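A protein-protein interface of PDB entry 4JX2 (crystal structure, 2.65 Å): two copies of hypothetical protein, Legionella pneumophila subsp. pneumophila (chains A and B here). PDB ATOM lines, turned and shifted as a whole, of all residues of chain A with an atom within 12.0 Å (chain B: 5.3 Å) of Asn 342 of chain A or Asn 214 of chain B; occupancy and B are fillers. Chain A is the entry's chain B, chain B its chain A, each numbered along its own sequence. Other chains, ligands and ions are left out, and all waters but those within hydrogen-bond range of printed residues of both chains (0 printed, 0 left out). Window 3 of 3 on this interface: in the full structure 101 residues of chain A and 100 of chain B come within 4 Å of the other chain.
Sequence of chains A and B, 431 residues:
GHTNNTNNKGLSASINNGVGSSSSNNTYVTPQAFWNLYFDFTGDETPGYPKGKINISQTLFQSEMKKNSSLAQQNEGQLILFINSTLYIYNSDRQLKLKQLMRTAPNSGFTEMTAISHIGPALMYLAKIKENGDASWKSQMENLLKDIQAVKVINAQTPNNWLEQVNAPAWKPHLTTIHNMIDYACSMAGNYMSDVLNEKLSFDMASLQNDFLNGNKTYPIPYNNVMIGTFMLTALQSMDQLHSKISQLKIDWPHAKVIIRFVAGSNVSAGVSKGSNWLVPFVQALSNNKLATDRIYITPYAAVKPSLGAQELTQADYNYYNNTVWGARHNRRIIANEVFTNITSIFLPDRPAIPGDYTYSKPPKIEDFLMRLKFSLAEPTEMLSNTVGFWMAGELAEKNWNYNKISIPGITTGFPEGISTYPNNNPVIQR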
ATOM      1  N   ILE A 334     -18.389  23.551  13.788  1.00  0.00           N
ATOM      2  CA  ILE A 334     -19.571  23.172  13.020  1.00  0.00           C
ATOM      3  C   ILE A 334     -19.286  23.316  11.520  1.00  0.00           C
ATOM      4  O   ILE A 334     -19.568  22.387  10.755  1.00  0.00           O
ATOM      5  CB  ILE A 334     -20.799  24.012  13.473  1.00  0.00           C
ATOM      6  CG1 ILE A 334     -21.148  23.771  14.957  1.00  0.00           C
ATOM      7  CG2 ILE A 334     -22.017  23.754  12.577  1.00  0.00           C
ATOM      8  CD1 ILE A 334     -22.082  24.892  15.568  1.00  0.00           C
ATOM      9  N   ILE A 335     -18.734  24.471  11.100  1.00  0.00           N
ATOM     10  CA  ILE A 335     -18.489  24.759   9.680  1.00  0.00           C
ATOM     11  C   ILE A 335     -17.518  23.737   9.075  1.00  0.00           C
ATOM     12  O   ILE A 335     -17.842  23.165   8.038  1.00  0.00           O
ATOM     13  CB  ILE A 335     -18.052  26.231   9.442  1.00  0.00           C
ATOM     14  CG1 ILE A 335     -19.232  27.202   9.774  1.00  0.00           C
ATOM     15  CG2 ILE A 335     -17.576  26.424   7.995  1.00  0.00           C
ATOM     16  CD1 ILE A 335     -18.844  28.596  10.086  1.00  0.00           C
ATOM     17  N   ALA A 336     -16.395  23.445   9.760  1.00  0.00           N
ATOM     18  CA  ALA A 336     -15.405  22.472   9.290  1.00  0.00           C
ATOM     19  C   ALA A 336     -16.004  21.082   9.076  1.00  0.00           C
ATOM     20  O   ALA A 336     -15.729  20.459   8.052  1.00  0.00           O
ATOM     21  CB  ALA A 336     -14.264  22.385  10.267  1.00  0.00           C
ATOM     22  N   ASN A 337     -16.850  20.621  10.014  1.00  0.00           N
ATOM     23  CA  ASN A 337     -17.465  19.308   9.912  1.00  0.00           C
ATOM     24  C   ASN A 337     -18.612  19.270   8.924  1.00  0.00           C
ATOM     25  O   ASN A 337     -18.738  18.270   8.228  1.00  0.00           O
ATOM     26  CB  ASN A 337     -17.903  18.790  11.266  1.00  0.00           C
ATOM     27  CG  ASN A 337     -16.738  18.249  12.043  1.00  0.00           C
ATOM     28  OD1 ASN A 337     -16.073  18.979  12.782  1.00  0.00           O
ATOM     29  ND2 ASN A 337     -16.417  16.970  11.834  1.00  0.00           N
ATOM     30  N   GLU A 338     -19.412  20.341   8.812  1.00  0.00           N
ATOM     31  CA  GLU A 338     -20.528  20.379   7.861  1.00  0.00           C
ATOM     32  C   GLU A 338     -20.049  20.559   6.419  1.00  0.00           C
ATOM     33  O   GLU A 338     -20.699  20.027   5.504  1.00  0.00           O
ATOM     34  CB  GLU A 338     -21.511  21.508   8.202  1.00  0.00           C
ATOM     35  CG  GLU A 338     -22.395  21.238   9.407  1.00  0.00           C
ATOM     36  CD  GLU A 338     -23.485  22.261   9.685  1.00  0.00           C
ATOM     37  OE1 GLU A 338     -23.663  23.204   8.879  1.00  0.00           O
ATOM     38  OE2 GLU A 338     -24.184  22.099  10.712  1.00  0.00           O
ATOM     39  N   VAL A 339     -18.948  21.330   6.194  1.00  0.00           N
ATOM     40  CA  VAL A 339     -18.474  21.563   4.828  1.00  0.00           C
ATOM     41  C   VAL A 339     -17.472  20.477   4.336  1.00  0.00           C
ATOM     42  O   VAL A 339     -17.589  20.065   3.193  1.00  0.00           O
ATOM     43  CB  VAL A 339     -17.925  22.991   4.566  1.00  0.00           C
ATOM     44  CG1 VAL A 339     -16.584  23.228   5.254  1.00  0.00           C
ATOM     45  CG2 VAL A 339     -17.774  23.225   3.070  1.00  0.00           C
ATOM     46  N   PHE A 340     -16.498  20.043   5.155  1.00  0.00           N
ATOM     47  CA  PHE A 340     -15.472  19.111   4.716  1.00  0.00           C
ATOM     48  C   PHE A 340     -15.849  17.632   4.935  1.00  0.00           C
ATOM     49  O   PHE A 340     -14.984  16.820   5.279  1.00  0.00           O
ATOM     50  CB  PHE A 340     -14.155  19.434   5.424  1.00  0.00           C
ATOM     51  CG  PHE A 340     -13.416  20.665   4.952  1.00  0.00           C
ATOM     52  CD1 PHE A 340     -13.082  20.825   3.605  1.00  0.00           C
ATOM     53  CD2 PHE A 340     -12.920  21.590   5.871  1.00  0.00           C
ATOM     54  CE1 PHE A 340     -12.344  21.927   3.181  1.00  0.00           C
ATOM     55  CE2 PHE A 340     -12.176  22.684   5.447  1.00  0.00           C
ATOM     56  CZ  PHE A 340     -11.876  22.836   4.109  1.00  0.00           C
ATOM     57  N   THR A 341     -17.097  17.257   4.636  1.00  0.00           N
ATOM     58  CA  THR A 341     -17.561  15.873   4.819  1.00  0.00           C
ATOM     59  C   THR A 341     -16.821  14.824   3.949  1.00  0.00           C
ATOM     60  O   THR A 341     -16.851  13.646   4.291  1.00  0.00           O
ATOM     61  CB  THR A 341     -19.062  15.765   4.563  1.00  0.00           C
ATOM     62  OG1 THR A 341     -19.335  16.074   3.183  1.00  0.00           O
ATOM     63  CG2 THR A 341     -19.901  16.624   5.546  1.00  0.00           C
ATOM     64  N   ASN A 342     -16.142  15.247   2.879  1.00  0.00           N
ATOM     65  CA  ASN A 342     -15.450  14.352   1.943  1.00  0.00           C
ATOM     66  C   ASN A 342     -14.026  14.086   2.349  1.00  0.00           C
ATOM     67  O   ASN A 342     -13.357  13.262   1.717  1.00  0.00           O
ATOM     68  CB  ASN A 342     -15.473  14.924   0.521  1.00  0.00           C
ATOM     69  CG  ASN A 342     -16.776  14.772  -0.196  1.00  0.00           C
ATOM     70  OD1 ASN A 342     -17.606  13.909   0.119  1.00  0.00           O
ATOM     71  ND2 ASN A 342     -16.907  15.509  -1.281  1.00  0.00           N
ATOM     72  N   ILE A 343     -13.552  14.797   3.379  1.00  0.00           N
ATOM     73  CA  ILE A 343     -12.211  14.677   3.952  1.00  0.00           C
ATOM     74  C   ILE A 343     -12.343  13.885   5.266  1.00  0.00           C
ATOM     75  O   ILE A 343     -13.163  14.241   6.134  1.00  0.00           O
ATOM     76  CB  ILE A 343     -11.638  16.105   4.145  1.00  0.00           C
ATOM     77  CG1 ILE A 343     -11.380  16.761   2.775  1.00  0.00           C
ATOM     78  CG2 ILE A 343     -10.389  16.122   5.041  1.00  0.00           C
ATOM     79  CD1 ILE A 343     -11.061  18.228   2.850  1.00  0.00           C
ATOM     80  N   THR A 344     -11.531  12.810   5.404  1.00  0.00           N
ATOM     81  CA  THR A 344     -11.483  11.928   6.575  1.00  0.00           C
ATOM     82  C   THR A 344     -11.181  12.755   7.793  1.00  0.00           C
ATOM     83  O   THR A 344     -10.342  13.669   7.735  1.00  0.00           O
ATOM     84  CB  THR A 344     -10.446  10.847   6.341  1.00  0.00           C
ATOM     85  OG1 THR A 344     -10.810  10.111   5.165  1.00  0.00           O
ATOM     86  CG2 THR A 344     -10.270   9.918   7.533  1.00  0.00           C
ATOM     87  N   SER A 345     -11.931  12.501   8.874  1.00  0.00           N
ATOM     88  CA  SER A 345     -11.749  13.224  10.128  1.00  0.00           C
ATOM     89  C   SER A 345     -10.639  12.602  10.948  1.00  0.00           C
ATOM     90  O   SER A 345     -10.571  11.377  11.094  1.00  0.00           O
ATOM     91  CB  SER A 345     -13.042  13.247  10.934  1.00  0.00           C
ATOM     92  OG  SER A 345     -13.943  14.180  10.379  1.00  0.00           O
ATOM     93  N   ILE A 346      -9.794  13.466  11.513  1.00  0.00           N
ATOM     94  CA  ILE A 346      -8.713  13.110  12.411  1.00  0.00           C
ATOM     95  C   ILE A 346      -9.225  13.281  13.815  1.00  0.00           C
ATOM     96  O   ILE A 346      -9.954  14.242  14.092  1.00  0.00           O
ATOM     97  CB  ILE A 346      -7.465  14.011  12.131  1.00  0.00           C
ATOM     98  CG1 ILE A 346      -6.810  13.662  10.776  1.00  0.00           C
ATOM     99  CG2 ILE A 346      -6.431  13.995  13.297  1.00  0.00           C
ATOM    100  CD1 ILE A 346      -5.699  14.616  10.323  1.00  0.00           C
ATOM    101  N   PHE A 347      -8.848  12.351  14.705  1.00  0.00           N
ATOM    102  CA  PHE A 347      -9.120  12.453  16.135  1.00  0.00           C
ATOM    103  C   PHE A 347      -7.796  12.229  16.870  1.00  0.00           C
ATOM    104  O   PHE A 347      -7.115  11.246  16.594  1.00  0.00           O
ATOM    105  CB  PHE A 347     -10.220  11.486  16.584  1.00  0.00           C
ATOM    106  CG  PHE A 347     -11.519  11.695  15.828  1.00  0.00           C
ATOM    107  CD1 PHE A 347     -12.444  12.640  16.254  1.00  0.00           C
ATOM    108  CD2 PHE A 347     -11.788  10.978  14.661  1.00  0.00           C
ATOM    109  CE1 PHE A 347     -13.596  12.891  15.516  1.00  0.00           C
ATOM    110  CE2 PHE A 347     -12.934  11.228  13.923  1.00  0.00           C
ATOM    111  CZ  PHE A 347     -13.834  12.179  14.356  1.00  0.00           C
ATOM    112  N   LEU B 208     -21.134  23.897  -1.903  1.00  0.00           N
ATOM    113  CA  LEU B 208     -19.834  24.578  -1.884  1.00  0.00           C
ATOM    114  C   LEU B 208     -18.676  23.563  -1.985  1.00  0.00           C
ATOM    115  O   LEU B 208     -17.741  23.770  -2.776  1.00  0.00           O
ATOM    116  CB  LEU B 208     -19.694  25.444  -0.613  1.00  0.00           C
ATOM    117  CG  LEU B 208     -18.305  26.009  -0.305  1.00  0.00           C
ATOM    118  CD1 LEU B 208     -17.924  27.155  -1.259  1.00  0.00           C
ATOM    119  CD2 LEU B 208     -18.224  26.431   1.116  1.00  0.00           C
ATOM    120  N   GLN B 209     -18.769  22.457  -1.217  1.00  0.00           N
ATOM    121  CA  GLN B 209     -17.764  21.419  -1.233  1.00  0.00           C
ATOM    122  C   GLN B 209     -17.662  20.767  -2.619  1.00  0.00           C
ATOM    123  O   GLN B 209     -16.568  20.680  -3.185  1.00  0.00           O
ATOM    124  CB  GLN B 209     -18.077  20.361  -0.165  1.00  0.00           C
ATOM    125  CG  GLN B 209     -17.108  19.182  -0.272  1.00  0.00           C
ATOM    126  CD  GLN B 209     -17.121  18.170   0.823  1.00  0.00           C
ATOM    127  OE1 GLN B 209     -16.070  17.830   1.358  1.00  0.00           O
ATOM    128  NE2 GLN B 209     -18.283  17.635   1.150  1.00  0.00           N
ATOM    129  N   ASN B 210     -18.803  20.311  -3.159  1.00  0.00           N
ATOM    130  CA  ASN B 210     -18.831  19.601  -4.431  1.00  0.00           C
ATOM    131  C   ASN B 210     -18.535  20.509  -5.641  1.00  0.00           C
ATOM    132  O   ASN B 210     -17.767  20.098  -6.511  1.00  0.00           O
ATOM    133  CB  ASN B 210     -20.186  18.916  -4.580  1.00  0.00           C
ATOM    134  CG  ASN B 210     -20.356  18.068  -5.808  1.00  0.00           C
ATOM    135  OD1 ASN B 210     -19.921  16.919  -5.871  1.00  0.00           O
ATOM    136  ND2 ASN B 210     -21.050  18.600  -6.789  1.00  0.00           N
ATOM    137  N   PHE B 212     -17.118  23.685  -5.776  1.00  0.00           N
ATOM    138  CA  PHE B 212     -15.954  24.568  -5.730  1.00  0.00           C
ATOM    139  C   PHE B 212     -14.705  23.960  -5.027  1.00  0.00           C
ATOM    140  O   PHE B 212     -13.666  23.810  -5.673  1.00  0.00           O
ATOM    141  CB  PHE B 212     -16.363  25.895  -5.059  1.00  0.00           C
ATOM    142  CG  PHE B 212     -15.226  26.844  -4.787  1.00  0.00           C
ATOM    143  CD1 PHE B 212     -14.541  27.457  -5.834  1.00  0.00           C
ATOM    144  CD2 PHE B 212     -14.845  27.140  -3.485  1.00  0.00           C
ATOM    145  CE1 PHE B 212     -13.497  28.345  -5.578  1.00  0.00           C
ATOM    146  CE2 PHE B 212     -13.784  28.020  -3.236  1.00  0.00           C
ATOM    147  CZ  PHE B 212     -13.156  28.654  -4.286  1.00  0.00           C
ATOM    148  N   LEU B 213     -14.796  23.636  -3.730  1.00  0.00           N
ATOM    149  CA  LEU B 213     -13.648  23.132  -2.978  1.00  0.00           C
ATOM    150  C   LEU B 213     -13.015  21.887  -3.616  1.00  0.00           C
ATOM    151  O   LEU B 213     -11.794  21.810  -3.687  1.00  0.00           O
ATOM    152  CB  LEU B 213     -14.023  22.861  -1.508  1.00  0.00           C
ATOM    153  CG  LEU B 213     -14.482  24.073  -0.695  1.00  0.00           C
ATOM    154  CD1 LEU B 213     -14.949  23.661   0.679  1.00  0.00           C
ATOM    155  CD2 LEU B 213     -13.408  25.150  -0.623  1.00  0.00           C
ATOM    156  N   ASN B 214     -13.831  20.958  -4.126  1.00  0.00           N
ATOM    157  CA  ASN B 214     -13.366  19.702  -4.745  1.00  0.00           C
ATOM    158  C   ASN B 214     -13.006  19.845  -6.222  1.00  0.00           C
ATOM    159  O   ASN B 214     -12.417  18.926  -6.804  1.00  0.00           O
ATOM    160  CB  ASN B 214     -14.434  18.614  -4.594  1.00  0.00           C
ATOM    161  CG  ASN B 214     -14.601  18.137  -3.182  1.00  0.00           C
ATOM    162  OD1 ASN B 214     -15.622  17.535  -2.837  1.00  0.00           O
ATOM    163  ND2 ASN B 214     -13.601  18.384  -2.334  1.00  0.00           N
ATOM    164  N   GLY B 215     -13.368  20.979  -6.801  1.00  0.00           N
ATOM    165  CA  GLY B 215     -13.142  21.240  -8.210  1.00  0.00           C
ATOM    166  C   GLY B 215     -14.412  20.997  -8.997  1.00  0.00           C
ATOM    167  O   GLY B 215     -15.414  20.480  -8.466  1.00  0.00           O
ATOM    168  N   ASN B 216     -14.369  21.393 -10.269  1.00  0.00           N
ATOM    169  CA  ASN B 216     -15.469  21.266 -11.204  1.00  0.00           C
ATOM    170  C   ASN B 216     -14.896  21.060 -12.619  1.00  0.00           C
ATOM    171  O   ASN B 216     -13.681  21.159 -12.794  1.00  0.00           O
ATOM    172  CB  ASN B 216     -16.392  22.487 -11.117  1.00  0.00           C
ATOM    173  CG  ASN B 216     -15.728  23.817 -11.364  1.00  0.00           C
ATOM    174  OD1 ASN B 216     -15.251  24.109 -12.469  1.00  0.00           O
ATOM    175  ND2 ASN B 216     -15.764  24.684 -10.359  1.00  0.00           N
ATOM    176  N   PRO B 220     -10.609  21.967 -12.962  1.00  0.00           N
ATOM    177  CA  PRO B 220     -10.382  20.619 -12.399  1.00  0.00           C
ATOM    178  C   PRO B 220      -9.472  20.525 -11.178  1.00  0.00           C
ATOM    179  O   PRO B 220      -9.622  19.555 -10.439  1.00  0.00           O
ATOM    180  CB  PRO B 220      -9.782  19.838 -13.577  1.00  0.00           C
ATOM    181  CG  PRO B 220      -9.233  20.859 -14.468  1.00  0.00           C
ATOM    182  CD  PRO B 220     -10.152  22.020 -14.363  1.00  0.00           C
ATOM    183  N   ILE B 221      -8.539  21.475 -10.971  1.00  0.00           N
ATOM    184  CA  ILE B 221      -7.695  21.477  -9.776  1.00  0.00           C
ATOM    185  C   ILE B 221      -8.576  21.968  -8.621  1.00  0.00           C
ATOM    186  O   ILE B 221      -9.079  23.096  -8.676  1.00  0.00           O
ATOM    187  CB  ILE B 221      -6.396  22.316  -9.918  1.00  0.00           C
ATOM    188  CG1 ILE B 221      -5.529  21.838 -11.099  1.00  0.00           C
ATOM    189  CG2 ILE B 221      -5.596  22.298  -8.600  1.00  0.00           C
ATOM    190  CD1 ILE B 221      -4.703  22.966 -11.760  1.00  0.00           C
ATOM    191  N   PRO B 222      -8.813  21.149  -7.577  1.00  0.00           N
ATOM    192  CA  PRO B 222      -9.649  21.627  -6.455  1.00  0.00           C
ATOM    193  C   PRO B 222      -9.133  22.929  -5.842  1.00  0.00           C
ATOM    194  O   PRO B 222      -7.918  23.144  -5.817  1.00  0.00           O
ATOM    195  CB  PRO B 222      -9.532  20.497  -5.423  1.00  0.00           C
ATOM    196  CG  PRO B 222      -9.162  19.300  -6.206  1.00  0.00           C
ATOM    197  CD  PRO B 222      -8.321  19.775  -7.348  1.00  0.00           C
ATOM    198  N   TYR B 223     -10.038  23.770  -5.284  1.00  0.00           N
ATOM    199  CA  TYR B 223      -9.604  24.965  -4.554  1.00  0.00           C
ATOM    200  C   TYR B 223      -8.869  24.532  -3.279  1.00  0.00           C
ATOM    201  O   TYR B 223      -8.023  25.277  -2.779  1.00  0.00           O
ATOM    202  CB  TYR B 223     -10.749  25.934  -4.224  1.00  0.00           C
ATOM    203  CG  TYR B 223     -10.200  27.315  -3.956  1.00  0.00           C
ATOM    204  CD1 TYR B 223      -9.853  28.162  -5.007  1.00  0.00           C
ATOM    205  CD2 TYR B 223      -9.939  27.745  -2.655  1.00  0.00           C
ATOM    206  CE1 TYR B 223      -9.279  29.411  -4.770  1.00  0.00           C
ATOM    207  CE2 TYR B 223      -9.357  28.991  -2.406  1.00  0.00           C
ATOM    208  CZ  TYR B 223      -9.028  29.817  -3.468  1.00  0.00           C
ATOM    209  OH  TYR B 223      -8.472  31.049  -3.241  1.00  0.00           O
ATOM    210  N   ASN B 224      -9.169  23.302  -2.784  1.00  0.00           N
ATOM    211  CA  ASN B 224      -8.494  22.654  -1.664  1.00  0.00           C
ATOM    212  C   ASN B 224      -6.966  22.677  -1.890  1.00  0.00           C
ATOM    213  O   ASN B 224      -6.229  22.978  -0.958  1.00  0.00           O
ATOM    214  CB  ASN B 224      -8.980  21.212  -1.542  1.00  0.00           C
ATOM    215  CG  ASN B 224     -10.351  20.956  -0.944  1.00  0.00           C
ATOM    216  OD1 ASN B 224     -10.866  21.672  -0.093  1.00  0.00           O
ATOM    217  ND2 ASN B 224     -10.925  19.828  -1.295  1.00  0.00           N
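Of the 13 printed residues of chain B, 5 touch a printed residue of chain A. Printed residues of chain B that touch a printed residue of chain A: Leu 208, Gln 209, Leu 213, Asn 214 and Asn 224. Hydrophobic or aromatic side chains of chain B within 4 Å of the printed part of chain A: Leu 208 and Leu 213. Hydrophobic or aromatic side chains of chain A that line the printed part of chain B: Val 339 and Phe 340. Among the printed residues, 8 pairs touch across the chains.
Of the printed residues of chain B, Val 339 of chain A touches Leu 208, Gln 209 and Leu 213. Of the printed residues of chain B, Thr 341 of chain A touches Gln 209. Asn 342 of chain A touches just these residues of chain B: Gln 209 and Asn 214. Thr 344 of chain A touches none of the printed residues of chain B. Of the printed residues of chain A, Leu 208 of chain B touches Val 339 (3.8 Å). Gln 209 of chain B touches just these residues of chain A: Val 339 (3.1 Å), Phe 340 (3.6 Å), Thr 341 (2.8 Å) and Asn 342 (3.0 Å). No residue of chain A comes within 4 Å of Asn 210 of chain B. No residue of chain A comes within 4 Å of Phe 212 of chain B. Of the printed residues of chain A, Leu 213 of chain B touches Val 339. Asn 214 of chain B touches just one residue of chain A: Asn 342. No residue of chain A comes within 4 Å of Asn 216 of chain B. No residue of chain A comes within 4 Å of Pro 222 of chain B. Printed residues of chain A within 4 Å of Asn 224 of chain B: Phe 340. The nearest printed residue of chain B that does not touch Asn 342 of chain A is Asn 210 of chain B (5.5 Å). The nearest residue of chain A that does not touch Asn 214 of chain B is Ile 343 of chain A (5.8 Å).
Leu 208 of chain B touches Val 339 of chain A. CG2 of Val 339 of chain A touches CD1 of Leu 213 of chain B, 3.7 Å away. C of Phe 340 of chain A touches OE1 of Gln 209 of chain B, at 3.6 Å. Phe 340 of chain A touches Asn 224 of chain B (CE1 to OD1, 3.6 Å).
No position is printed for both chains.
The backbone NH (N) of Leu 213 of chain B sits at hydrogen-bond distance from the backbone carbonyl oxygen (O) of Leu 208 of chain B. The backbone carbonyl oxygen (O) of Gln 209 of chain B is in hydrogen-bond range of the backbone NH (N) of Asn 214 of chain B. The backbone carbonyl oxygen (O) of Leu 213 of chain B is in hydrogen-bond range of the backbone NH (N) of Tyr 223 of chain B (3.1 Å). N of Asn 224 of chain B is in hydrogen-bond range of O of Leu 213 of chain B (3.2 Å). The side-chain amide nitrogen (ND2) of Asn 214 of chain B lies close to the side-chain amide nitrogen (ND2) of Asn 224 of chain B (3.2 Å).
The side-chain amide nitrogen of Gln 209 of chain B lies close to the backbone carbonyl oxygen of Val 339 of chain A (3.2 Å). The side-chain amide nitrogen (NE2) of Gln 209 of chain B is in hydrogen-bond range of the side-chain hydroxyl (OG1) of Thr 341 of chain A. OE1 of Gln 209 of chain B is in hydrogen-bond range of N of Asn 342 of chain A (3.0 Å). OD1 of Asn 214 of chain B sits at hydrogen-bond distance from ND2 of Asn 342 of chain A, at 2.9 Å.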
